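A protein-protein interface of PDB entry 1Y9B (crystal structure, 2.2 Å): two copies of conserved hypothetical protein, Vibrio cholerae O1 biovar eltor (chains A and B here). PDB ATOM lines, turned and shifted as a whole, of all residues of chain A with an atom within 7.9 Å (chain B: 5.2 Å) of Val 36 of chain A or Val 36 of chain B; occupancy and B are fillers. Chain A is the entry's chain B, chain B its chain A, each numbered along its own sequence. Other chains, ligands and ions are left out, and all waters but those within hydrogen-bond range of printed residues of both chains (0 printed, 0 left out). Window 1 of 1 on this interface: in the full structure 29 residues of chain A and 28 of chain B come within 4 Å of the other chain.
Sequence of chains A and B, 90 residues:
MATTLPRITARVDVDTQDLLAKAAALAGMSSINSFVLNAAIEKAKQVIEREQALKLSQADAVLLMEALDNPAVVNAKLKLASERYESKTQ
The side-chain hydroxyl (OG1) of Thr 9 of chain A lies close to the backbone carbonyl oxygen (O) of Ile 8 of chain B (3.3 Å). The backbone NH (N) of Ile 8 of chain B sits at hydrogen-bond distance from the backbone carbonyl oxygen (O) of Ala 10 of chain A, at 2.8 Å. The backbone NH of Thr 9 of chain A lies within hydrogen-bond range of the side-chain amide oxygen of Asn 33 of chain B.
Val 36 of chain A touches just these residues of chain B: Ile 8, Val 36 and Ala 40. Of chain A, only Ile 8, Val 36 and Ala 40 come within 4 Å of Val 36 of chain B. Of the printed residues of chain B, Phe 35 of chain A touches Ala 40 (3.4 Å). Of the printed residues of chain B, Val 12 of chain A touches Ile 8. Of the printed residues of chain B, Thr 9 of chain A touches Ile 8 and Asn 33. Of the printed residues of chain B, Ile 8 of chain A touches Ile 8 (3.9 Å), Leu 20 (3.9 Å), Ile 32 (3.7 Å), Asn 33 (3.5 Å) and Val 36 (3.7 Å). Of the printed residues of chain A, Phe 35 of chain B touches Ala 40 (3.5 Å) and Lys 43 (3.8 Å). Ser 34 of chain B touches none of the printed residues of chain A. The nearest printed residue of chain B that does not touch Val 36 of chain A is Leu 37 of chain B (5.3 Å). The nearest residue of chain A that does not touch Val 36 of chain B is Leu 37 of chain A (5.4 Å). The nearest printed residue of chain A that does not touch Phe 35 of chain B is Ile 41 of chain A (5.6 Å).
Of the 23 printed residues of chain A, 13 touch a printed residue of chain B. Printed residues of chain A that touch a printed residue of chain B: Ile 8, Thr 9, Ala 10, Val 12, Thr 16, Leu 20, Ile 32, Asn 33, Phe 35, Val 36, Ala 39, Ala 40 and Lys 43. Hydrophobic or aromatic side chains of chain B that line the printed part of chain A: Ile 8, Leu 20, Ile 32, Phe 35, Val 36, Ala 39, Ala 40 and Ile 41. Among the printed residues, no Asp or Glu carboxylate lies within 4 Å of a Lys or Arg side-chain nitrogen of the other chain.
Ile 8 of chain B touches Ile 8 of chain A (O to O, 3.9 Å). Ile 8 of chain A touches Leu 20 of chain B. Asn 33 of chain B touches Ile 8 of chain A. Ala 40 of chain B touches Leu 20 of chain A. CG2 of Ile 32 of chain A touches CG1 of Ile 8 of chain B (3.96 Å). OD1 of Asn 33 of chain A touches CA of Ile 8 of chain B (3.4 Å). Val 36 of chain A touches Ile 8 of chain B (CG1 to CG2, 3.6 Å). Val 36 of chain A touches Ala 40 of chain B. Ala 39 of chain A touches Ala 39 of chain B. Lys 43 of chain A touches Phe 35 of chain B.
Ile 8 of chain A touches Leu 20 of chain B, and with the chains exchanged Leu 20 of chain A touches Ile 8 of chain B. Ile 8 of chain A touches Ile 32 of chain B, and with the chains exchanged Ile 32 of chain A touches Ile 8 of chain B. Ile 8 of chain A touches Val 36 of chain B, and with the chains exchanged Val 36 of chain A touches Ile 8 of chain B. Phe 35 of chain A touches Ala 40 of chain B, and with the chains exchanged Ala 40 of chain A touches Phe 35 of chain B. Positions printed for both chains: 8, 20, 32, 33, 34, 35, 36, 37, 38, 39, 40 and 41. Of the 26 pairs that touch across the chains among the printed residues, 19 have their exchanged pair printed and touching as well.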
ATOM      1  N   ARG A   7     -21.832 -28.825   7.280  1.00  0.00           N
ATOM      2  CA  ARG A   7     -20.850 -29.738   7.888  1.00  0.00           C
ATOM      3  C   ARG A   7     -19.432 -29.187   7.681  1.00  0.00           C
ATOM      4  O   ARG A   7     -19.033 -28.945   6.545  1.00  0.00           O
ATOM      5  CB  ARG A   7     -20.960 -31.121   7.223  1.00  0.00           C
ATOM      6  CG  ARG A   7     -20.369 -32.286   7.992  1.00  0.00           C
ATOM      7  CD  ARG A   7     -21.445 -33.054   8.770  1.00  0.00           C
ATOM      8  NE  ARG A   7     -20.851 -33.841   9.856  1.00  0.00           N
ATOM      9  CZ  ARG A   7     -21.507 -34.333  10.909  1.00  0.00           C
ATOM     10  NH1 ARG A   7     -22.822 -34.148  11.049  1.00  0.00           N
ATOM     11  NH2 ARG A   7     -20.835 -35.016  11.835  1.00  0.00           N
ATOM     12  N   ILE A   8     -18.671 -28.981   8.750  1.00  0.00           N
ATOM     13  CA  ILE A   8     -17.225 -28.724   8.574  1.00  0.00           C
ATOM     14  C   ILE A   8     -16.457 -30.050   8.541  1.00  0.00           C
ATOM     15  O   ILE A   8     -16.715 -30.958   9.335  1.00  0.00           O
ATOM     16  CB  ILE A   8     -16.615 -27.720   9.603  1.00  0.00           C
ATOM     17  CG1 ILE A   8     -16.837 -28.180  11.047  1.00  0.00           C
ATOM     18  CG2 ILE A   8     -17.192 -26.327   9.386  1.00  0.00           C
ATOM     19  CD1 ILE A   8     -15.733 -27.780  11.996  1.00  0.00           C
ATOM     20  N   THR A   9     -15.538 -30.168   7.595  1.00  0.00           N
ATOM     21  CA  THR A   9     -14.884 -31.439   7.331  1.00  0.00           C
ATOM     22  C   THR A   9     -13.482 -31.221   6.767  1.00  0.00           C
ATOM     23  O   THR A   9     -13.285 -30.383   5.882  1.00  0.00           O
ATOM     24  CB  THR A   9     -15.730 -32.338   6.384  1.00  0.00           C
ATOM     25  OG1 THR A   9     -14.978 -33.505   6.035  1.00  0.00           O
ATOM     26  CG2 THR A   9     -16.101 -31.604   5.114  1.00  0.00           C
ATOM     27  N   ALA A  10     -12.510 -31.968   7.281  1.00  0.00           N
ATOM     28  CA  ALA A  10     -11.131 -31.847   6.814  1.00  0.00           C
ATOM     29  C   ALA A  10     -10.341 -33.142   6.941  1.00  0.00           C
ATOM     30  O   ALA A  10     -10.470 -33.875   7.921  1.00  0.00           O
ATOM     31  CB  ALA A  10     -10.407 -30.695   7.544  1.00  0.00           C
ATOM     32  N   VAL A  12      -6.909 -34.978   7.751  1.00  0.00           N
ATOM     33  CA  VAL A  12      -5.654 -34.800   8.498  1.00  0.00           C
ATOM     34  C   VAL A  12      -4.653 -35.892   8.153  1.00  0.00           C
ATOM     35  O   VAL A  12      -5.026 -37.055   7.921  1.00  0.00           O
ATOM     36  CB  VAL A  12      -5.836 -34.756  10.062  1.00  0.00           C
ATOM     37  CG1 VAL A  12      -6.673 -33.577  10.464  1.00  0.00           C
ATOM     38  CG2 VAL A  12      -6.422 -36.060  10.601  1.00  0.00           C
ATOM     39  N   THR A  16      -0.557 -33.776  11.826  1.00  0.00           N
ATOM     40  CA  THR A  16      -1.641 -32.898  12.252  1.00  0.00           C
ATOM     41  C   THR A  16      -2.511 -33.593  13.285  1.00  0.00           C
ATOM     42  O   THR A  16      -2.860 -32.994  14.298  1.00  0.00           O
ATOM     43  CB  THR A  16      -2.484 -32.455  11.033  1.00  0.00           C
ATOM     44  OG1 THR A  16      -1.612 -31.891  10.055  1.00  0.00           O
ATOM     45  CG2 THR A  16      -3.510 -31.407  11.406  1.00  0.00           C
ATOM     46  N   LEU A  20      -3.140 -32.253  16.969  1.00  0.00           N
ATOM     47  CA  LEU A  20      -4.503 -31.923  17.430  1.00  0.00           C
ATOM     48  C   LEU A  20      -4.965 -32.757  18.620  1.00  0.00           C
ATOM     49  O   LEU A  20      -5.759 -32.276  19.449  1.00  0.00           O
ATOM     50  CB  LEU A  20      -5.517 -32.000  16.303  1.00  0.00           C
ATOM     51  CG  LEU A  20      -5.235 -31.072  15.102  1.00  0.00           C
ATOM     52  CD1 LEU A  20      -6.221 -31.407  14.021  1.00  0.00           C
ATOM     53  CD2 LEU A  20      -5.273 -29.546  15.448  1.00  0.00           C
ATOM     54  N   ALA A  21      -4.488 -34.002  18.682  1.00  0.00           N
ATOM     55  CA  ALA A  21      -4.827 -34.933  19.772  1.00  0.00           C
ATOM     56  C   ALA A  21      -4.159 -34.541  21.077  1.00  0.00           C
ATOM     57  O   ALA A  21      -4.784 -34.649  22.114  1.00  0.00           O
ATOM     58  CB  ALA A  21      -4.452 -36.328  19.402  1.00  0.00           C
ATOM     59  N   ALA A  24      -5.965 -31.411  22.127  1.00  0.00           N
ATOM     60  CA  ALA A  24      -7.292 -31.788  22.665  1.00  0.00           C
ATOM     61  C   ALA A  24      -7.176 -32.403  24.072  1.00  0.00           C
ATOM     62  O   ALA A  24      -8.024 -32.175  24.937  1.00  0.00           O
ATOM     63  CB  ALA A  24      -8.051 -32.758  21.683  1.00  0.00           C
ATOM     64  N   MET A  29     -10.572 -31.726  26.098  1.00  0.00           N
ATOM     65  CA  MET A  29     -11.595 -32.184  25.127  1.00  0.00           C
ATOM     66  C   MET A  29     -11.493 -33.687  25.005  1.00  0.00           C
ATOM     67  O   MET A  29     -10.420 -34.251  25.221  1.00  0.00           O
ATOM     68  CB  MET A  29     -11.349 -31.600  23.729  1.00  0.00           C
ATOM     69  CG  MET A  29     -11.040 -30.125  23.682  1.00  0.00           C
ATOM     70  SD  MET A  29     -12.529 -29.133  23.824  1.00  0.00           S
ATOM     71  CE  MET A  29     -11.910 -27.626  23.134  1.00  0.00           C
ATOM     72  N   SER A  31     -12.632 -35.277  22.077  1.00  0.00           N
ATOM     73  CA  SER A  31     -12.413 -35.534  20.659  1.00  0.00           C
ATOM     74  C   SER A  31     -11.616 -34.437  19.953  1.00  0.00           C
ATOM     75  O   SER A  31     -11.635 -33.267  20.344  1.00  0.00           O
ATOM     76  CB  SER A  31     -13.745 -35.757  19.933  1.00  0.00           C
ATOM     77  OG  SER A  31     -14.566 -34.621  19.986  1.00  0.00           O
ATOM     78  N   ILE A  32     -10.907 -34.837  18.914  1.00  0.00           N
ATOM     79  CA  ILE A  32     -10.315 -33.897  17.977  1.00  0.00           C
ATOM     80  C   ILE A  32     -11.392 -32.965  17.385  1.00  0.00           C
ATOM     81  O   ILE A  32     -11.210 -31.753  17.376  1.00  0.00           O
ATOM     82  CB  ILE A  32      -9.482 -34.658  16.870  1.00  0.00           C
ATOM     83  CG1 ILE A  32      -8.170 -35.182  17.480  1.00  0.00           C
ATOM     84  CG2 ILE A  32      -9.214 -33.763  15.647  1.00  0.00           C
ATOM     85  CD1 ILE A  32      -7.296 -36.065  16.554  1.00  0.00           C
ATOM     86  N   ASN A  33     -12.520 -33.546  16.946  1.00  0.00           N
ATOM     87  CA  ASN A  33     -13.647 -32.836  16.309  1.00  0.00           C
ATOM     88  C   ASN A  33     -14.137 -31.661  17.139  1.00  0.00           C
ATOM     89  O   ASN A  33     -14.428 -30.568  16.614  1.00  0.00           O
ATOM     90  CB  ASN A  33     -14.847 -33.795  16.090  1.00  0.00           C
ATOM     91  CG  ASN A  33     -14.672 -34.747  14.900  1.00  0.00           C
ATOM     92  OD1 ASN A  33     -13.812 -34.555  14.023  1.00  0.00           O
ATOM     93  ND2 ASN A  33     -15.508 -35.784  14.862  1.00  0.00           N
ATOM     94  N   SER A  34     -14.283 -31.917  18.433  1.00  0.00           N
ATOM     95  CA  SER A  34     -14.624 -30.902  19.427  1.00  0.00           C
ATOM     96  C   SER A  34     -13.574 -29.821  19.568  1.00  0.00           C
ATOM     97  O   SER A  34     -13.896 -28.635  19.550  1.00  0.00           O
ATOM     98  CB  SER A  34     -14.832 -31.546  20.782  1.00  0.00           C
ATOM     99  OG  SER A  34     -16.214 -31.647  20.952  1.00  0.00           O
ATOM    100  N   PHE A  35     -12.323 -30.224  19.746  1.00  0.00           N
ATOM    101  CA  PHE A  35     -11.239 -29.267  19.748  1.00  0.00           C
ATOM    102  C   PHE A  35     -11.265 -28.335  18.512  1.00  0.00           C
ATOM    103  O   PHE A  35     -11.169 -27.110  18.624  1.00  0.00           O
ATOM    104  CB  PHE A  35      -9.879 -29.973  19.854  1.00  0.00           C
ATOM    105  CG  PHE A  35      -8.739 -29.007  19.814  1.00  0.00           C
ATOM    106  CD1 PHE A  35      -8.335 -28.352  20.982  1.00  0.00           C
ATOM    107  CD2 PHE A  35      -8.150 -28.649  18.583  1.00  0.00           C
ATOM    108  CE1 PHE A  35      -7.287 -27.391  20.939  1.00  0.00           C
ATOM    109  CE2 PHE A  35      -7.131 -27.697  18.522  1.00  0.00           C
ATOM    110  CZ  PHE A  35      -6.697 -27.060  19.702  1.00  0.00           C
ATOM    111  N   VAL A  36     -11.397 -28.936  17.338  1.00  0.00           N
ATOM    112  CA  VAL A  36     -11.348 -28.239  16.051  1.00  0.00           C
ATOM    113  C   VAL A  36     -12.472 -27.213  15.894  1.00  0.00           C
ATOM    114  O   VAL A  36     -12.213 -26.049  15.569  1.00  0.00           O
ATOM    115  CB  VAL A  36     -11.312 -29.270  14.875  1.00  0.00           C
ATOM    116  CG1 VAL A  36     -11.521 -28.602  13.506  1.00  0.00           C
ATOM    117  CG2 VAL A  36     -10.009 -30.069  14.913  1.00  0.00           C
ATOM    118  N   LEU A  37     -13.710 -27.642  16.119  1.00  0.00           N
ATOM    119  CA  LEU A  37     -14.868 -26.746  16.042  1.00  0.00           C
ATOM    120  C   LEU A  37     -14.723 -25.528  16.954  1.00  0.00           C
ATOM    121  O   LEU A  37     -14.917 -24.403  16.498  1.00  0.00           O
ATOM    122  CB  LEU A  37     -16.149 -27.490  16.386  1.00  0.00           C
ATOM    123  CG  LEU A  37     -17.411 -26.634  16.465  1.00  0.00           C
ATOM    124  CD1 LEU A  37     -17.790 -26.036  15.102  1.00  0.00           C
ATOM    125  CD2 LEU A  37     -18.581 -27.443  17.102  1.00  0.00           C
ATOM    126  N   ASN A  38     -14.386 -25.780  18.229  1.00  0.00           N
ATOM    127  CA  ASN A  38     -14.131 -24.732  19.218  1.00  0.00           C
ATOM    128  C   ASN A  38     -12.980 -23.780  18.855  1.00  0.00           C
ATOM    129  O   ASN A  38     -13.127 -22.563  19.003  1.00  0.00           O
ATOM    130  CB  ASN A  38     -13.902 -25.342  20.612  1.00  0.00           C
ATOM    131  CG  ASN A  38     -13.618 -24.270  21.692  1.00  0.00           C
ATOM    132  OD1 ASN A  38     -12.481 -23.767  21.834  1.00  0.00           O
ATOM    133  ND2 ASN A  38     -14.659 -23.921  22.462  1.00  0.00           N
ATOM    134  N   ALA A  39     -11.836 -24.339  18.434  1.00  0.00           N
ATOM    135  CA  ALA A  39     -10.733 -23.555  17.892  1.00  0.00           C
ATOM    136  C   ALA A  39     -11.168 -22.647  16.724  1.00  0.00           C
ATOM    137  O   ALA A  39     -10.705 -21.547  16.625  1.00  0.00           O
ATOM    138  CB  ALA A  39      -9.628 -24.456  17.461  1.00  0.00           C
ATOM    139  N   ALA A  40     -12.077 -23.119  15.867  1.00  0.00           N
ATOM    140  CA  ALA A  40     -12.519 -22.396  14.668  1.00  0.00           C
ATOM    141  C   ALA A  40     -13.425 -21.222  14.997  1.00  0.00           C
ATOM    142  O   ALA A  40     -13.323 -20.167  14.383  1.00  0.00           O
ATOM    143  CB  ALA A  40     -13.241 -23.332  13.730  1.00  0.00           C
ATOM    144  N   ILE A  41     -14.333 -21.444  15.943  1.00  0.00           N
ATOM    145  CA  ILE A  41     -15.282 -20.439  16.386  1.00  0.00           C
ATOM    146  C   ILE A  41     -14.574 -19.302  17.106  1.00  0.00           C
ATOM    147  O   ILE A  41     -14.859 -18.135  16.851  1.00  0.00           O
ATOM    148  CB  ILE A  41     -16.410 -21.070  17.254  1.00  0.00           C
ATOM    149  CG1 ILE A  41     -17.291 -21.986  16.398  1.00  0.00           C
ATOM    150  CG2 ILE A  41     -17.252 -20.011  17.944  1.00  0.00           C
ATOM    151  CD1 ILE A  41     -18.147 -22.915  17.265  1.00  0.00           C
ATOM    152  N   GLU A  42     -13.621 -19.645  17.968  1.00  0.00           N
ATOM    153  CA  GLU A  42     -12.820 -18.668  18.711  1.00  0.00           C
ATOM    154  C   GLU A  42     -11.986 -17.787  17.755  1.00  0.00           C
ATOM    155  O   GLU A  42     -11.972 -16.568  17.882  1.00  0.00           O
ATOM    156  CB  GLU A  42     -11.951 -19.426  19.712  1.00  0.00           C
ATOM    157  CG  GLU A  42     -11.202 -18.583  20.757  1.00  0.00           C
ATOM    158  CD  GLU A  42     -10.007 -19.333  21.408  1.00  0.00           C
ATOM    159  OE1 GLU A  42     -10.000 -20.598  21.474  1.00  0.00           O
ATOM    160  OE2 GLU A  42      -9.066 -18.635  21.853  1.00  0.00           O
ATOM    161  N   LYS A  43     -11.307 -18.413  16.801  1.00  0.00           N
ATOM    162  CA  LYS A  43     -10.597 -17.718  15.734  1.00  0.00           C
ATOM    163  C   LYS A  43     -11.493 -16.870  14.806  1.00  0.00           C
ATOM    164  O   LYS A  43     -11.110 -15.751  14.445  1.00  0.00           O
ATOM    165  CB  LYS A  43      -9.738 -18.718  14.931  1.00  0.00           C
ATOM    166  CG  LYS A  43      -8.859 -18.130  13.834  1.00  0.00           C
ATOM    167  CD  LYS A  43      -7.737 -17.186  14.322  1.00  0.00           C
ATOM    168  CE  LYS A  43      -6.818 -16.842  13.130  1.00  0.00           C
ATOM    169  NZ  LYS A  43      -5.712 -15.854  13.405  1.00  0.00           N
ATOM    170  N   ILE B   8     -11.672 -35.003  10.145  1.00  0.00           N
ATOM    171  CA  ILE B   8     -12.391 -34.074  11.008  1.00  0.00           C
ATOM    172  C   ILE B   8     -13.738 -33.774  10.369  1.00  0.00           C
ATOM    173  O   ILE B   8     -13.831 -33.600   9.145  1.00  0.00           O
ATOM    174  CB  ILE B   8     -11.659 -32.743  11.235  1.00  0.00           C
ATOM    175  CG1 ILE B   8     -10.315 -32.977  11.924  1.00  0.00           C
ATOM    176  CG2 ILE B   8     -12.549 -31.774  12.036  1.00  0.00           C
ATOM    177  CD1 ILE B   8      -9.359 -31.822  11.707  1.00  0.00           C
ATOM    178  N   LEU B  20     -18.116 -18.453  10.429  1.00  0.00           N
ATOM    179  CA  LEU B  20     -16.890 -18.997   9.854  1.00  0.00           C
ATOM    180  C   LEU B  20     -16.677 -18.550   8.393  1.00  0.00           C
ATOM    181  O   LEU B  20     -15.533 -18.365   7.923  1.00  0.00           O
ATOM    182  CB  LEU B  20     -16.894 -20.527   9.951  1.00  0.00           C
ATOM    183  CG  LEU B  20     -17.067 -21.265  11.278  1.00  0.00           C
ATOM    184  CD1 LEU B  20     -17.176 -22.794  11.022  1.00  0.00           C
ATOM    185  CD2 LEU B  20     -15.933 -20.932  12.256  1.00  0.00           C
ATOM    186  N   ILE B  32     -14.459 -22.486   4.215  1.00  0.00           N
ATOM    187  CA  ILE B  32     -14.591 -22.648   5.649  1.00  0.00           C
ATOM    188  C   ILE B  32     -13.697 -23.770   6.143  1.00  0.00           C
ATOM    189  O   ILE B  32     -13.094 -23.633   7.188  1.00  0.00           O
ATOM    190  CB  ILE B  32     -16.049 -22.947   6.037  1.00  0.00           C
ATOM    191  CG1 ILE B  32     -16.935 -21.776   5.661  1.00  0.00           C
ATOM    192  CG2 ILE B  32     -16.183 -23.221   7.549  1.00  0.00           C
ATOM    193  CD1 ILE B  32     -18.420 -22.076   5.871  1.00  0.00           C
ATOM    194  N   ASN B  33     -13.615 -24.872   5.395  1.00  0.00           N
ATOM    195  CA  ASN B  33     -12.870 -26.058   5.824  1.00  0.00           C
ATOM    196  C   ASN B  33     -11.394 -25.784   5.950  1.00  0.00           C
ATOM    197  O   ASN B  33     -10.728 -26.338   6.825  1.00  0.00           O
ATOM    198  CB  ASN B  33     -13.097 -27.225   4.862  1.00  0.00           C
ATOM    199  CG  ASN B  33     -14.493 -27.772   4.951  1.00  0.00           C
ATOM    200  OD1 ASN B  33     -15.159 -27.677   5.997  1.00  0.00           O
ATOM    201  ND2 ASN B  33     -14.969 -28.324   3.856  1.00  0.00           N
ATOM    202  N   SER B  34     -10.889 -24.933   5.061  1.00  0.00           N
ATOM    203  CA  SER B  34      -9.535 -24.401   5.155  1.00  0.00           C
ATOM    204  C   SER B  34      -9.283 -23.549   6.377  1.00  0.00           C
ATOM    205  O   SER B  34      -8.246 -23.671   7.020  1.00  0.00           O
ATOM    206  CB  SER B  34      -9.227 -23.546   3.949  1.00  0.00           C
ATOM    207  OG  SER B  34      -8.378 -24.294   3.129  1.00  0.00           O
ATOM    208  N   PHE B  35     -10.210 -22.639   6.625  1.00  0.00           N
ATOM    209  CA  PHE B  35     -10.155 -21.732   7.753  1.00  0.00           C
ATOM    210  C   PHE B  35     -10.135 -22.526   9.052  1.00  0.00           C
ATOM    211  O   PHE B  35      -9.348 -22.263   9.975  1.00  0.00           O
ATOM    212  CB  PHE B  35     -11.390 -20.814   7.731  1.00  0.00           C
ATOM    213  CG  PHE B  35     -11.479 -19.935   8.922  1.00  0.00           C
ATOM    214  CD1 PHE B  35     -10.749 -18.756   8.970  1.00  0.00           C
ATOM    215  CD2 PHE B  35     -12.232 -20.319  10.038  1.00  0.00           C
ATOM    216  CE1 PHE B  35     -10.790 -17.952  10.091  1.00  0.00           C
ATOM    217  CE2 PHE B  35     -12.260 -19.520  11.161  1.00  0.00           C
ATOM    218  CZ  PHE B  35     -11.538 -18.334  11.183  1.00  0.00           C
ATOM    219  N   VAL B  36     -11.056 -23.478   9.109  1.00  0.00           N
ATOM    220  CA  VAL B  36     -11.244 -24.355  10.243  1.00  0.00           C
ATOM    221  C   VAL B  36      -9.964 -25.134  10.575  1.00  0.00           C
ATOM    222  O   VAL B  36      -9.520 -25.108  11.718  1.00  0.00           O
ATOM    223  CB  VAL B  36     -12.436 -25.295   9.974  1.00  0.00           C
ATOM    224  CG1 VAL B  36     -12.494 -26.412  10.990  1.00  0.00           C
ATOM    225  CG2 VAL B  36     -13.733 -24.486  10.008  1.00  0.00           C
ATOM    226  N   LEU B  37      -9.383 -25.821   9.589  1.00  0.00           N
ATOM    227  CA  LEU B  37      -8.179 -26.590   9.815  1.00  0.00           C
ATOM    228  C   LEU B  37      -6.990 -25.722  10.218  1.00  0.00           C
ATOM    229  O   LEU B  37      -6.220 -26.109  11.082  1.00  0.00           O
ATOM    230  CB  LEU B  37      -7.806 -27.405   8.572  1.00  0.00           C
ATOM    231  CG  LEU B  37      -6.557 -28.303   8.609  1.00  0.00           C
ATOM    232  CD1 LEU B  37      -6.649 -29.406   9.671  1.00  0.00           C
ATOM    233  CD2 LEU B  37      -6.331 -28.921   7.246  1.00  0.00           C
ATOM    234  N   ASN B  38      -6.809 -24.585   9.551  1.00  0.00           N
ATOM    235  CA  ASN B  38      -5.744 -23.658   9.910  1.00  0.00           C
ATOM    236  C   ASN B  38      -5.951 -23.009  11.283  1.00  0.00           C
ATOM    237  O   ASN B  38      -4.969 -22.842  12.010  1.00  0.00           O
ATOM    238  CB  ASN B  38      -5.563 -22.568   8.868  1.00  0.00           C
ATOM    239  CG  ASN B  38      -4.505 -21.559   9.289  1.00  0.00           C
ATOM    240  OD1 ASN B  38      -4.808 -20.525   9.914  1.00  0.00           O
ATOM    241  ND2 ASN B  38      -3.242 -21.890   9.018  1.00  0.00           N
ATOM    242  N   ALA B  39      -7.203 -22.648  11.620  1.00  0.00           N
ATOM    243  CA  ALA B  39      -7.600 -22.248  12.987  1.00  0.00           C
ATOM    244  C   ALA B  39      -7.256 -23.312  14.037  1.00  0.00           C
ATOM    245  O   ALA B  39      -6.673 -23.001  15.071  1.00  0.00           O
ATOM    246  CB  ALA B  39      -9.090 -21.905  13.062  1.00  0.00           C
ATOM    247  N   ALA B  40      -7.614 -24.564  13.774  1.00  0.00           N
ATOM    248  CA  ALA B  40      -7.329 -25.656  14.684  1.00  0.00           C
ATOM    249  C   ALA B  40      -5.824 -25.910  14.885  1.00  0.00           C
ATOM    250  O   ALA B  40      -5.375 -26.135  15.997  1.00  0.00           O
ATOM    251  CB  ALA B  40      -8.030 -26.917  14.204  1.00  0.00           C
ATOM    252  N   ILE B  41      -5.051 -25.902  13.803  1.00  0.00           N
ATOM    253  CA  ILE B  41      -3.613 -26.109  13.890  1.00  0.00           C
ATOM    254  C   ILE B  41      -2.893 -25.010  14.694  1.00  0.00           C
ATOM    255  O   ILE B  41      -1.992 -25.328  15.490  1.00  0.00           O
ATOM    256  CB  ILE B  41      -2.986 -26.325  12.477  1.00  0.00           C
ATOM    257  CG1 ILE B  41      -3.388 -27.694  11.906  1.00  0.00           C
ATOM    258  CG2 ILE B  41      -1.436 -26.164  12.466  1.00  0.00           C
ATOM    259  CD1 ILE B  41      -3.132 -27.822  10.366  1.00  0.00           C
